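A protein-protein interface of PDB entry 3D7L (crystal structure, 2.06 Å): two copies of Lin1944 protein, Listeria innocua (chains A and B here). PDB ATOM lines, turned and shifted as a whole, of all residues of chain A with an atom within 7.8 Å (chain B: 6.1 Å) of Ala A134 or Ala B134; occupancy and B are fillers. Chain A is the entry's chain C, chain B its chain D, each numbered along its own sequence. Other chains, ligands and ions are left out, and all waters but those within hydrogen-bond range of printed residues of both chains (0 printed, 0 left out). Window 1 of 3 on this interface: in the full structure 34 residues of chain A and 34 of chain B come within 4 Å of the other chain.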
ATOM      1  N   ILE A  86      16.545   6.481 -33.771  1.00  0.00           N
ATOM      2  CA  ILE A  86      16.669   7.417 -32.665  1.00  0.00           C
ATOM      3  C   ILE A  86      15.465   7.326 -31.713  1.00  0.00           C
ATOM      4  O   ILE A  86      15.621   7.409 -30.487  1.00  0.00           O
ATOM      5  CB  ILE A  86      16.895   8.877 -33.210  1.00  0.00           C
ATOM      6  CG1 ILE A  86      18.349   9.042 -33.674  1.00  0.00           C
ATOM      7  CG2 ILE A  86      16.563   9.934 -32.167  1.00  0.00           C
ATOM      8  CD1 ILE A  86      18.594  10.213 -34.606  1.00  0.00           C
ATOM      9  N   LYS A  89      15.301   2.170 -30.965  1.00  0.00           N
ATOM     10  CA  LYS A  89      16.392   1.414 -30.326  1.00  0.00           C
ATOM     11  C   LYS A  89      17.282   2.282 -29.423  1.00  0.00           C
ATOM     12  O   LYS A  89      17.848   1.789 -28.431  1.00  0.00           O
ATOM     13  CB  LYS A  89      17.207   0.587 -31.333  1.00  0.00           C
ATOM     14  CG  LYS A  89      18.486   0.026 -30.772  1.00  0.00           C
ATOM     15  CD  LYS A  89      18.723  -1.407 -31.198  1.00  0.00           C
ATOM     16  CE  LYS A  89      19.306  -2.223 -30.041  1.00  0.00           C
ATOM     17  NZ  LYS A  89      20.377  -3.128 -30.553  1.00  0.00           N
ATOM     18  N   LEU A  90      17.397   3.572 -29.757  1.00  0.00           N
ATOM     19  CA  LEU A  90      18.223   4.494 -28.973  1.00  0.00           C
ATOM     20  C   LEU A  90      17.393   5.190 -27.902  1.00  0.00           C
ATOM     21  O   LEU A  90      17.595   4.959 -26.712  1.00  0.00           O
ATOM     22  CB  LEU A  90      18.881   5.538 -29.881  1.00  0.00           C
ATOM     23  CG  LEU A  90      19.973   6.459 -29.324  1.00  0.00           C
ATOM     24  CD1 LEU A  90      20.678   7.097 -30.524  1.00  0.00           C
ATOM     25  CD2 LEU A  90      19.455   7.527 -28.361  1.00  0.00           C
ATOM     26  N   GLY A  91      16.484   6.059 -28.336  1.00  0.00           N
ATOM     27  CA  GLY A  91      15.685   6.900 -27.438  1.00  0.00           C
ATOM     28  C   GLY A  91      14.672   6.142 -26.611  1.00  0.00           C
ATOM     29  O   GLY A  91      14.474   6.463 -25.438  1.00  0.00           O
ATOM     30  N   ILE A  94      16.546   4.326 -23.870  1.00  0.00           N
ATOM     31  CA  ILE A  94      17.050   5.243 -22.857  1.00  0.00           C
ATOM     32  C   ILE A  94      15.884   5.783 -22.023  1.00  0.00           C
ATOM     33  O   ILE A  94      16.012   5.879 -20.816  1.00  0.00           O
ATOM     34  CB  ILE A  94      18.008   6.299 -23.416  1.00  0.00           C
ATOM     35  CG1 ILE A  94      19.286   5.569 -23.883  1.00  0.00           C
ATOM     36  CG2 ILE A  94      18.335   7.357 -22.347  1.00  0.00           C
ATOM     37  CD1 ILE A  94      20.320   6.418 -24.612  1.00  0.00           C
ATOM     38  N   LEU A 112      19.889  -3.246 -20.729  1.00  0.00           N
ATOM     39  CA  LEU A 112      19.481  -2.849 -22.090  1.00  0.00           C
ATOM     40  C   LEU A 112      20.261  -3.601 -23.173  1.00  0.00           C
ATOM     41  O   LEU A 112      21.341  -4.133 -22.908  1.00  0.00           O
ATOM     42  CB  LEU A 112      19.630  -1.340 -22.294  1.00  0.00           C
ATOM     43  CG  LEU A 112      19.069  -0.408 -21.210  1.00  0.00           C
ATOM     44  CD1 LEU A 112      19.486   1.038 -21.490  1.00  0.00           C
ATOM     45  CD2 LEU A 112      17.570  -0.562 -21.124  1.00  0.00           C
ATOM     46  N   THR A 114      22.269  -3.864 -26.870  1.00  0.00           N
ATOM     47  CA  THR A 114      23.060  -3.147 -27.873  1.00  0.00           C
ATOM     48  C   THR A 114      23.326  -4.112 -29.037  1.00  0.00           C
ATOM     49  O   THR A 114      22.369  -4.561 -29.671  1.00  0.00           O
ATOM     50  CB  THR A 114      24.331  -2.475 -27.258  1.00  0.00           C
ATOM     51  OG1 THR A 114      25.161  -3.448 -26.627  1.00  0.00           O
ATOM     52  CG2 THR A 114      23.933  -1.416 -26.188  1.00  0.00           C
ATOM     53  N   MET A 118      28.288  -2.071 -33.478  1.00  0.00           N
ATOM     54  CA  MET A 118      29.071  -0.926 -33.012  1.00  0.00           C
ATOM     55  C   MET A 118      30.569  -1.169 -33.087  1.00  0.00           C
ATOM     56  O   MET A 118      31.327  -0.243 -33.410  1.00  0.00           O
ATOM     57  CB  MET A 118      28.657  -0.474 -31.604  1.00  0.00           C
ATOM     58  CG  MET A 118      28.950  -1.475 -30.513  1.00  0.00           C
ATOM     59  SD  MET A 118      28.466  -0.800 -28.758  1.00  0.00           S
ATOM     60  CE  MET A 118      28.755  -2.450 -27.772  1.00  0.00           C
ATOM     61  N   ALA A 126      25.093   1.472 -40.158  1.00  0.00           N
ATOM     62  CA  ALA A 126      25.525   2.702 -39.458  1.00  0.00           C
ATOM     63  C   ALA A 126      24.529   3.180 -38.404  1.00  0.00           C
ATOM     64  O   ALA A 126      24.922   3.664 -37.329  1.00  0.00           O
ATOM     65  CB  ALA A 126      25.785   3.787 -40.431  1.00  0.00           C
ATOM     66  N   SER A 127      23.252   3.028 -38.729  1.00  0.00           N
ATOM     67  CA  SER A 127      22.166   3.503 -37.886  1.00  0.00           C
ATOM     68  C   SER A 127      22.034   2.650 -36.644  1.00  0.00           C
ATOM     69  O   SER A 127      21.988   3.179 -35.525  1.00  0.00           O
ATOM     70  CB  SER A 127      20.857   3.554 -38.673  1.00  0.00           C
ATOM     71  OG  SER A 127      19.888   4.294 -37.980  1.00  0.00           O
ATOM     72  N   ALA A 128      22.020   1.327 -36.834  1.00  0.00           N
ATOM     73  CA  ALA A 128      22.126   0.391 -35.697  1.00  0.00           C
ATOM     74  C   ALA A 128      23.382   0.628 -34.856  1.00  0.00           C
ATOM     75  O   ALA A 128      23.309   0.583 -33.618  1.00  0.00           O
ATOM     76  CB  ALA A 128      22.064  -1.068 -36.178  1.00  0.00           C
ATOM     77  N   ALA A 129      24.515   0.900 -35.513  1.00  0.00           N
ATOM     78  CA  ALA A 129      25.774   1.145 -34.807  1.00  0.00           C
ATOM     79  C   ALA A 129      25.660   2.344 -33.885  1.00  0.00           C
ATOM     80  O   ALA A 129      26.009   2.258 -32.704  1.00  0.00           O
ATOM     81  CB  ALA A 129      26.956   1.367 -35.810  1.00  0.00           C
ATOM     82  N   MET A 130      25.195   3.468 -34.440  1.00  0.00           N
ATOM     83  CA  MET A 130      24.863   4.667 -33.677  1.00  0.00           C
ATOM     84  C   MET A 130      24.089   4.360 -32.365  1.00  0.00           C
ATOM     85  O   MET A 130      24.507   4.805 -31.289  1.00  0.00           O
ATOM     86  CB  MET A 130      24.038   5.624 -34.551  1.00  0.00           C
ATOM     87  CG  MET A 130      23.648   6.894 -33.864  1.00  0.00           C
ATOM     88  SD  MET A 130      22.220   7.877 -34.749  1.00  0.00           S
ATOM     89  CE  MET A 130      20.731   6.539 -34.595  1.00  0.00           C
ATOM     90  N   ALA A 131      22.978   3.616 -32.480  1.00  0.00           N
ATOM     91  CA  ALA A 131      22.119   3.296 -31.350  1.00  0.00           C
ATOM     92  C   ALA A 131      22.877   2.483 -30.329  1.00  0.00           C
ATOM     93  O   ALA A 131      22.783   2.738 -29.132  1.00  0.00           O
ATOM     94  CB  ALA A 131      20.885   2.541 -31.805  1.00  0.00           C
ATOM     95  N   ASN A 132      23.614   1.489 -30.807  1.00  0.00           N
ATOM     96  CA  ASN A 132      24.380   0.615 -29.924  1.00  0.00           C
ATOM     97  C   ASN A 132      25.441   1.377 -29.138  1.00  0.00           C
ATOM     98  O   ASN A 132      25.588   1.163 -27.925  1.00  0.00           O
ATOM     99  CB  ASN A 132      24.988  -0.543 -30.723  1.00  0.00           C
ATOM    100  CG  ASN A 132      23.923  -1.464 -31.304  1.00  0.00           C
ATOM    101  OD1 ASN A 132      22.776  -1.445 -30.887  1.00  0.00           O
ATOM    102  ND2 ASN A 132      24.305  -2.269 -32.284  1.00  0.00           N
ATOM    103  N   GLY A 133      26.164   2.268 -29.813  1.00  0.00           N
ATOM    104  CA  GLY A 133      27.134   3.145 -29.151  1.00  0.00           C
ATOM    105  C   GLY A 133      26.524   4.032 -28.070  1.00  0.00           C
ATOM    106  O   GLY A 133      27.058   4.137 -26.972  1.00  0.00           O
ATOM    107  N   ALA A 134      25.410   4.665 -28.419  1.00  0.00           N
ATOM    108  CA  ALA A 134      24.636   5.559 -27.564  1.00  0.00           C
ATOM    109  C   ALA A 134      24.161   4.873 -26.278  1.00  0.00           C
ATOM    110  O   ALA A 134      24.385   5.383 -25.174  1.00  0.00           O
ATOM    111  CB  ALA A 134      23.423   6.075 -28.351  1.00  0.00           C
ATOM    112  N   VAL A 135      23.509   3.723 -26.428  1.00  0.00           N
ATOM    113  CA  VAL A 135      23.008   2.985 -25.291  1.00  0.00           C
ATOM    114  C   VAL A 135      24.164   2.474 -24.417  1.00  0.00           C
ATOM    115  O   VAL A 135      24.089   2.595 -23.185  1.00  0.00           O
ATOM    116  CB  VAL A 135      22.024   1.874 -25.719  1.00  0.00           C
ATOM    117  CG1 VAL A 135      21.534   1.063 -24.484  1.00  0.00           C
ATOM    118  CG2 VAL A 135      20.808   2.499 -26.439  1.00  0.00           C
ATOM    119  N   THR A 136      25.254   1.978 -25.037  1.00  0.00           N
ATOM    120  CA  THR A 136      26.422   1.500 -24.274  1.00  0.00           C
ATOM    121  C   THR A 136      27.005   2.594 -23.369  1.00  0.00           C
ATOM    122  O   THR A 136      27.211   2.381 -22.159  1.00  0.00           O
ATOM    123  CB  THR A 136      27.555   0.922 -25.208  1.00  0.00           C
ATOM    124  OG1 THR A 136      27.001  -0.092 -26.056  1.00  0.00           O
ATOM    125  CG2 THR A 136      28.695   0.306 -24.401  1.00  0.00           C
ATOM    126  N   ALA A 137      27.309   3.745 -23.969  1.00  0.00           N
ATOM    127  CA  ALA A 137      27.893   4.896 -23.264  1.00  0.00           C
ATOM    128  C   ALA A 137      26.968   5.527 -22.193  1.00  0.00           C
ATOM    129  O   ALA A 137      27.441   5.878 -21.093  1.00  0.00           O
ATOM    130  CB  ALA A 137      28.359   5.949 -24.281  1.00  0.00           C
ATOM    131  N   PHE A 138      25.683   5.713 -22.542  1.00  0.00           N
ATOM    132  CA  PHE A 138      24.668   6.192 -21.601  1.00  0.00           C
ATOM    133  C   PHE A 138      24.632   5.321 -20.336  1.00  0.00           C
ATOM    134  O   PHE A 138      24.564   5.869 -19.238  1.00  0.00           O
ATOM    135  CB  PHE A 138      23.251   6.245 -22.200  1.00  0.00           C
ATOM    136  CG  PHE A 138      22.168   6.512 -21.152  1.00  0.00           C
ATOM    137  CD1 PHE A 138      21.945   7.800 -20.673  1.00  0.00           C
ATOM    138  CD2 PHE A 138      21.456   5.472 -20.584  1.00  0.00           C
ATOM    139  CE1 PHE A 138      20.996   8.050 -19.679  1.00  0.00           C
ATOM    140  CE2 PHE A 138      20.478   5.710 -19.597  1.00  0.00           C
ATOM    141  CZ  PHE A 138      20.246   6.986 -19.148  1.00  0.00           C
ATOM    142  N   ALA A 139      24.650   3.996 -20.501  1.00  0.00           N
ATOM    143  CA  ALA A 139      24.648   3.044 -19.372  1.00  0.00           C
ATOM    144  C   ALA A 139      25.924   3.082 -18.556  1.00  0.00           C
ATOM    145  O   ALA A 139      25.882   2.973 -17.318  1.00  0.00           O
ATOM    146  CB  ALA A 139      24.395   1.637 -19.837  1.00  0.00           C
ATOM    147  N   LYS A 140      27.059   3.233 -19.236  1.00  0.00           N
ATOM    148  CA  LYS A 140      28.335   3.310 -18.527  1.00  0.00           C
ATOM    149  C   LYS A 140      28.335   4.532 -17.583  1.00  0.00           C
ATOM    150  O   LYS A 140      28.740   4.430 -16.421  1.00  0.00           O
ATOM    151  CB  LYS A 140      29.526   3.384 -19.500  1.00  0.00           C
ATOM    152  CG  LYS A 140      30.863   3.236 -18.772  1.00  0.00           C
ATOM    153  CD  LYS A 140      32.040   3.629 -19.622  1.00  0.00           C
ATOM    154  CE  LYS A 140      33.386   3.120 -19.068  1.00  0.00           C
ATOM    155  NZ  LYS A 140      33.463   2.924 -17.581  1.00  0.00           N
ATOM    156  N   THR A 154      24.547  -3.292 -20.028  1.00  0.00           N
ATOM    157  CA  THR A 154      24.061  -3.619 -21.361  1.00  0.00           C
ATOM    158  C   THR A 154      24.557  -4.996 -21.830  1.00  0.00           C
ATOM    159  O   THR A 154      25.569  -5.528 -21.357  1.00  0.00           O
ATOM    160  CB  THR A 154      24.458  -2.534 -22.397  1.00  0.00           C
ATOM    161  OG1 THR A 154      25.875  -2.320 -22.353  1.00  0.00           O
ATOM    162  CG2 THR A 154      23.739  -1.221 -22.116  1.00  0.00           C
ATOM    163  N   LEU B  90      24.380  14.992 -30.758  1.00  0.00           N
ATOM    164  CA  LEU B  90      24.172  13.674 -31.373  1.00  0.00           C
ATOM    165  C   LEU B  90      23.680  13.797 -32.822  1.00  0.00           C
ATOM    166  O   LEU B  90      24.437  13.568 -33.766  1.00  0.00           O
ATOM    167  CB  LEU B  90      23.204  12.815 -30.547  1.00  0.00           C
ATOM    168  CG  LEU B  90      23.134  11.304 -30.869  1.00  0.00           C
ATOM    169  CD1 LEU B  90      22.582  10.535 -29.656  1.00  0.00           C
ATOM    170  CD2 LEU B  90      22.326  10.992 -32.122  1.00  0.00           C
ATOM    171  N   ILE B  94      25.531  14.112 -36.715  1.00  0.00           N
ATOM    172  CA  ILE B  94      25.317  13.003 -37.646  1.00  0.00           C
ATOM    173  C   ILE B  94      24.659  13.481 -38.937  1.00  0.00           C
ATOM    174  O   ILE B  94      25.084  13.092 -40.045  1.00  0.00           O
ATOM    175  CB  ILE B  94      24.630  11.784 -36.955  1.00  0.00           C
ATOM    176  CG1 ILE B  94      25.679  11.089 -36.038  1.00  0.00           C
ATOM    177  CG2 ILE B  94      24.092  10.794 -37.991  1.00  0.00           C
ATOM    178  CD1 ILE B  94      25.154  10.112 -35.046  1.00  0.00           C
ATOM    179  N   ALA B 129      27.625  11.684 -22.552  1.00  0.00           N
ATOM    180  CA  ALA B 129      28.171  10.338 -22.752  1.00  0.00           C
ATOM    181  C   ALA B 129      27.453   9.590 -23.902  1.00  0.00           C
ATOM    182  O   ALA B 129      28.094   9.109 -24.838  1.00  0.00           O
ATOM    183  CB  ALA B 129      28.066   9.523 -21.442  1.00  0.00           C
ATOM    184  N   MET B 130      26.121   9.510 -23.814  1.00  0.00           N
ATOM    185  CA  MET B 130      25.264   9.004 -24.910  1.00  0.00           C
ATOM    186  C   MET B 130      25.619   9.563 -26.289  1.00  0.00           C
ATOM    187  O   MET B 130      25.865   8.803 -27.233  1.00  0.00           O
ATOM    188  CB  MET B 130      23.790   9.323 -24.595  1.00  0.00           C
ATOM    189  CG  MET B 130      22.756   8.780 -25.603  1.00  0.00           C
ATOM    190  SD  MET B 130      21.011   9.713 -25.457  1.00  0.00           S
ATOM    191  CE  MET B 130      21.534  11.492 -25.983  1.00  0.00           C
ATOM    192  N   ALA B 131      25.617  10.896 -26.398  1.00  0.00           N
ATOM    193  CA  ALA B 131      25.926  11.584 -27.646  1.00  0.00           C
ATOM    194  C   ALA B 131      27.302  11.165 -28.136  1.00  0.00           C
ATOM    195  O   ALA B 131      27.467  10.832 -29.306  1.00  0.00           O
ATOM    196  CB  ALA B 131      25.887  13.102 -27.461  1.00  0.00           C
ATOM    197  N   ASN B 132      28.296  11.195 -27.247  1.00  0.00           N
ATOM    198  CA  ASN B 132      29.673  10.828 -27.632  1.00  0.00           C
ATOM    199  C   ASN B 132      29.818   9.383 -28.116  1.00  0.00           C
ATOM    200  O   ASN B 132      30.500   9.114 -29.117  1.00  0.00           O
ATOM    201  CB  ASN B 132      30.671  11.109 -26.502  1.00  0.00           C
ATOM    202  CG  ASN B 132      30.759  12.570 -26.158  1.00  0.00           C
ATOM    203  OD1 ASN B 132      30.283  13.432 -26.918  1.00  0.00           O
ATOM    204  ND2 ASN B 132      31.305  12.869 -24.983  1.00  0.00           N
ATOM    205  N   GLY B 133      29.191   8.458 -27.397  1.00  0.00           N
ATOM    206  CA  GLY B 133      29.180   7.058 -27.793  1.00  0.00           C
ATOM    207  C   GLY B 133      28.494   6.859 -29.139  1.00  0.00           C
ATOM    208  O   GLY B 133      28.981   6.108 -29.994  1.00  0.00           O
ATOM    209  N   ALA B 134      27.382   7.557 -29.329  1.00  0.00           N
ATOM    210  CA  ALA B 134      26.601   7.459 -30.544  1.00  0.00           C
ATOM    211  C   ALA B 134      27.424   7.913 -31.753  1.00  0.00           C
ATOM    212  O   ALA B 134      27.460   7.248 -32.788  1.00  0.00           O
ATOM    213  CB  ALA B 134      25.367   8.299 -30.422  1.00  0.00           C
ATOM    214  N   VAL B 135      28.087   9.046 -31.599  1.00  0.00           N
ATOM    215  CA  VAL B 135      28.858   9.647 -32.693  1.00  0.00           C
ATOM    216  C   VAL B 135      30.098   8.794 -33.018  1.00  0.00           C
ATOM    217  O   VAL B 135      30.461   8.610 -34.210  1.00  0.00           O
ATOM    218  CB  VAL B 135      29.162  11.148 -32.392  1.00  0.00           C
ATOM    219  CG1 VAL B 135      30.165  11.752 -33.397  1.00  0.00           C
ATOM    220  CG2 VAL B 135      27.837  11.972 -32.434  1.00  0.00           C
ATOM    221  N   THR B 136      30.694   8.199 -31.978  1.00  0.00           N
ATOM    222  CA  THR B 136      31.908   7.380 -32.148  1.00  0.00           C
ATOM    223  C   THR B 136      31.556   6.166 -33.004  1.00  0.00           C
ATOM    224  O   THR B 136      32.220   5.890 -34.028  1.00  0.00           O
ATOM    225  CB  THR B 136      32.512   6.922 -30.788  1.00  0.00           C
ATOM    226  OG1 THR B 136      32.922   8.062 -30.018  1.00  0.00           O
ATOM    227  CG2 THR B 136      33.702   6.033 -30.984  1.00  0.00           C
ATOM    228  N   ALA B 137      30.499   5.475 -32.590  1.00  0.00           N
ATOM    229  CA  ALA B 137      30.025   4.257 -33.257  1.00  0.00           C
ATOM    230  C   ALA B 137      29.503   4.504 -34.671  1.00  0.00           C
ATOM    231  O   ALA B 137      29.789   3.710 -35.565  1.00  0.00           O
ATOM    232  CB  ALA B 137      28.969   3.572 -32.419  1.00  0.00           C
ATOM    233  N   PHE B 138      28.733   5.569 -34.867  1.00  0.00           N
ATOM    234  CA  PHE B 138      28.286   5.984 -36.219  1.00  0.00           C
ATOM    235  C   PHE B 138      29.461   6.140 -37.186  1.00  0.00           C
ATOM    236  O   PHE B 138      29.461   5.568 -38.268  1.00  0.00           O
ATOM    237  CB  PHE B 138      27.483   7.304 -36.204  1.00  0.00           C
ATOM    238  CG  PHE B 138      27.178   7.847 -37.599  1.00  0.00           C
ATOM    239  CD1 PHE B 138      26.158   7.275 -38.378  1.00  0.00           C
ATOM    240  CD2 PHE B 138      27.937   8.894 -38.152  1.00  0.00           C
ATOM    241  CE1 PHE B 138      25.881   7.755 -39.683  1.00  0.00           C
ATOM    242  CE2 PHE B 138      27.683   9.376 -39.450  1.00  0.00           C
ATOM    243  CZ  PHE B 138      26.644   8.809 -40.224  1.00  0.00           C
ATOM    244  N   ALA B 139      30.453   6.910 -36.773  1.00  0.00           N
ATOM    245  CA  ALA B 139      31.661   7.186 -37.573  1.00  0.00           C
ATOM    246  C   ALA B 139      32.469   5.929 -37.927  1.00  0.00           C
ATOM    247  O   ALA B 139      32.904   5.769 -39.074  1.00  0.00           O
ATOM    248  CB  ALA B 139      32.552   8.187 -36.836  1.00  0.00           C
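Printed residues of chain B within 4 Å of Met A130: Ile B94 (3.7 Å) and Ala B134 (3.5 Å). Of the printed residues of chain B, Gly A133 touches Gly B133, Ala B134 and Ala B137. Ala A134 touches just these residues of chain B: Met B130 (3.5 Å), Gly B133 (3.9 Å) and Ala B134 (3.6 Å). Printed residues of chain A within 4 Å of Gly B133: Gly A133, Ala A134 and Ala A137. Of chain A, only Met A130, Gly A133 and Ala A134 come within 4 Å of Ala B134. The nearest residue of chain A that does not touch Ala B134 is Leu A90 (4.8 Å).
Printed residues of chain A that touch a printed residue of chain B: Leu A90, Ile A94, Ala A126, Ala A129, Met A130, Gly A133, Ala A134, Ala A137 and Phe A138. Hydrophobic or aromatic side chains of chain A that line the printed part of chain B: Leu A90, Ile A94, Ala A129, Met A130, Ala A134, Ala A137 and Phe A138. Of the 13 printed residues of chain B, 7 touch a printed residue of chain A. Among the printed residues, 15 pairs touch across the chains. Among the printed residues, no Asp or Glu carboxylate lies within 4 Å of a Lys or Arg side-chain nitrogen of the other chain.
Among the printed residues, merely in contact across the chains: Leu A90 with Met B130 (3.95 Å), Ile A94 with Met B130 (3.5 Å), Ala A126 with Phe B138 (3.96 Å), Ala A129 with Ala B137 (3.3 Å), Met A130 with Ile B94 (3.7 Å), Met A130 with Ala B134 (3.5 Å), Gly A133 with Gly B133 (3.6 Å), Gly A133 with Ala B134 (3.8 Å), Gly A133 with Ala B137 (3.8 Å), Ala A134 with Met B130 (3.5 Å), Ala A134 with Gly B133 (3.9 Å), Ala A134 with Ala B134 (3.6 Å), Ala A137 with Ala B129 (3.2 Å), Ala A137 with Gly B133 (3.8 Å) and Phe A138 with Met B130 (3.9 Å).
Ile A94 touches Met B130, and with the chains exchanged Met A130 touches Ile B94. Met A130 touches Ala B134, and with the chains exchanged Ala A134 touches Met B130. Ala A134 touches its own counterpart, Ala B134. Phe A138 touches Met B130, but with the chains exchanged Met A130 does not touch Phe B138 (4.1 Å). Positions printed for both chains: 90, 94, 129, 130, 131, 132, 133, 134, 135, 136, 137, 138 and 139. Of the 15 pairs that touch across the chains among the printed residues, 12 have their exchanged pair printed and touching as well.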
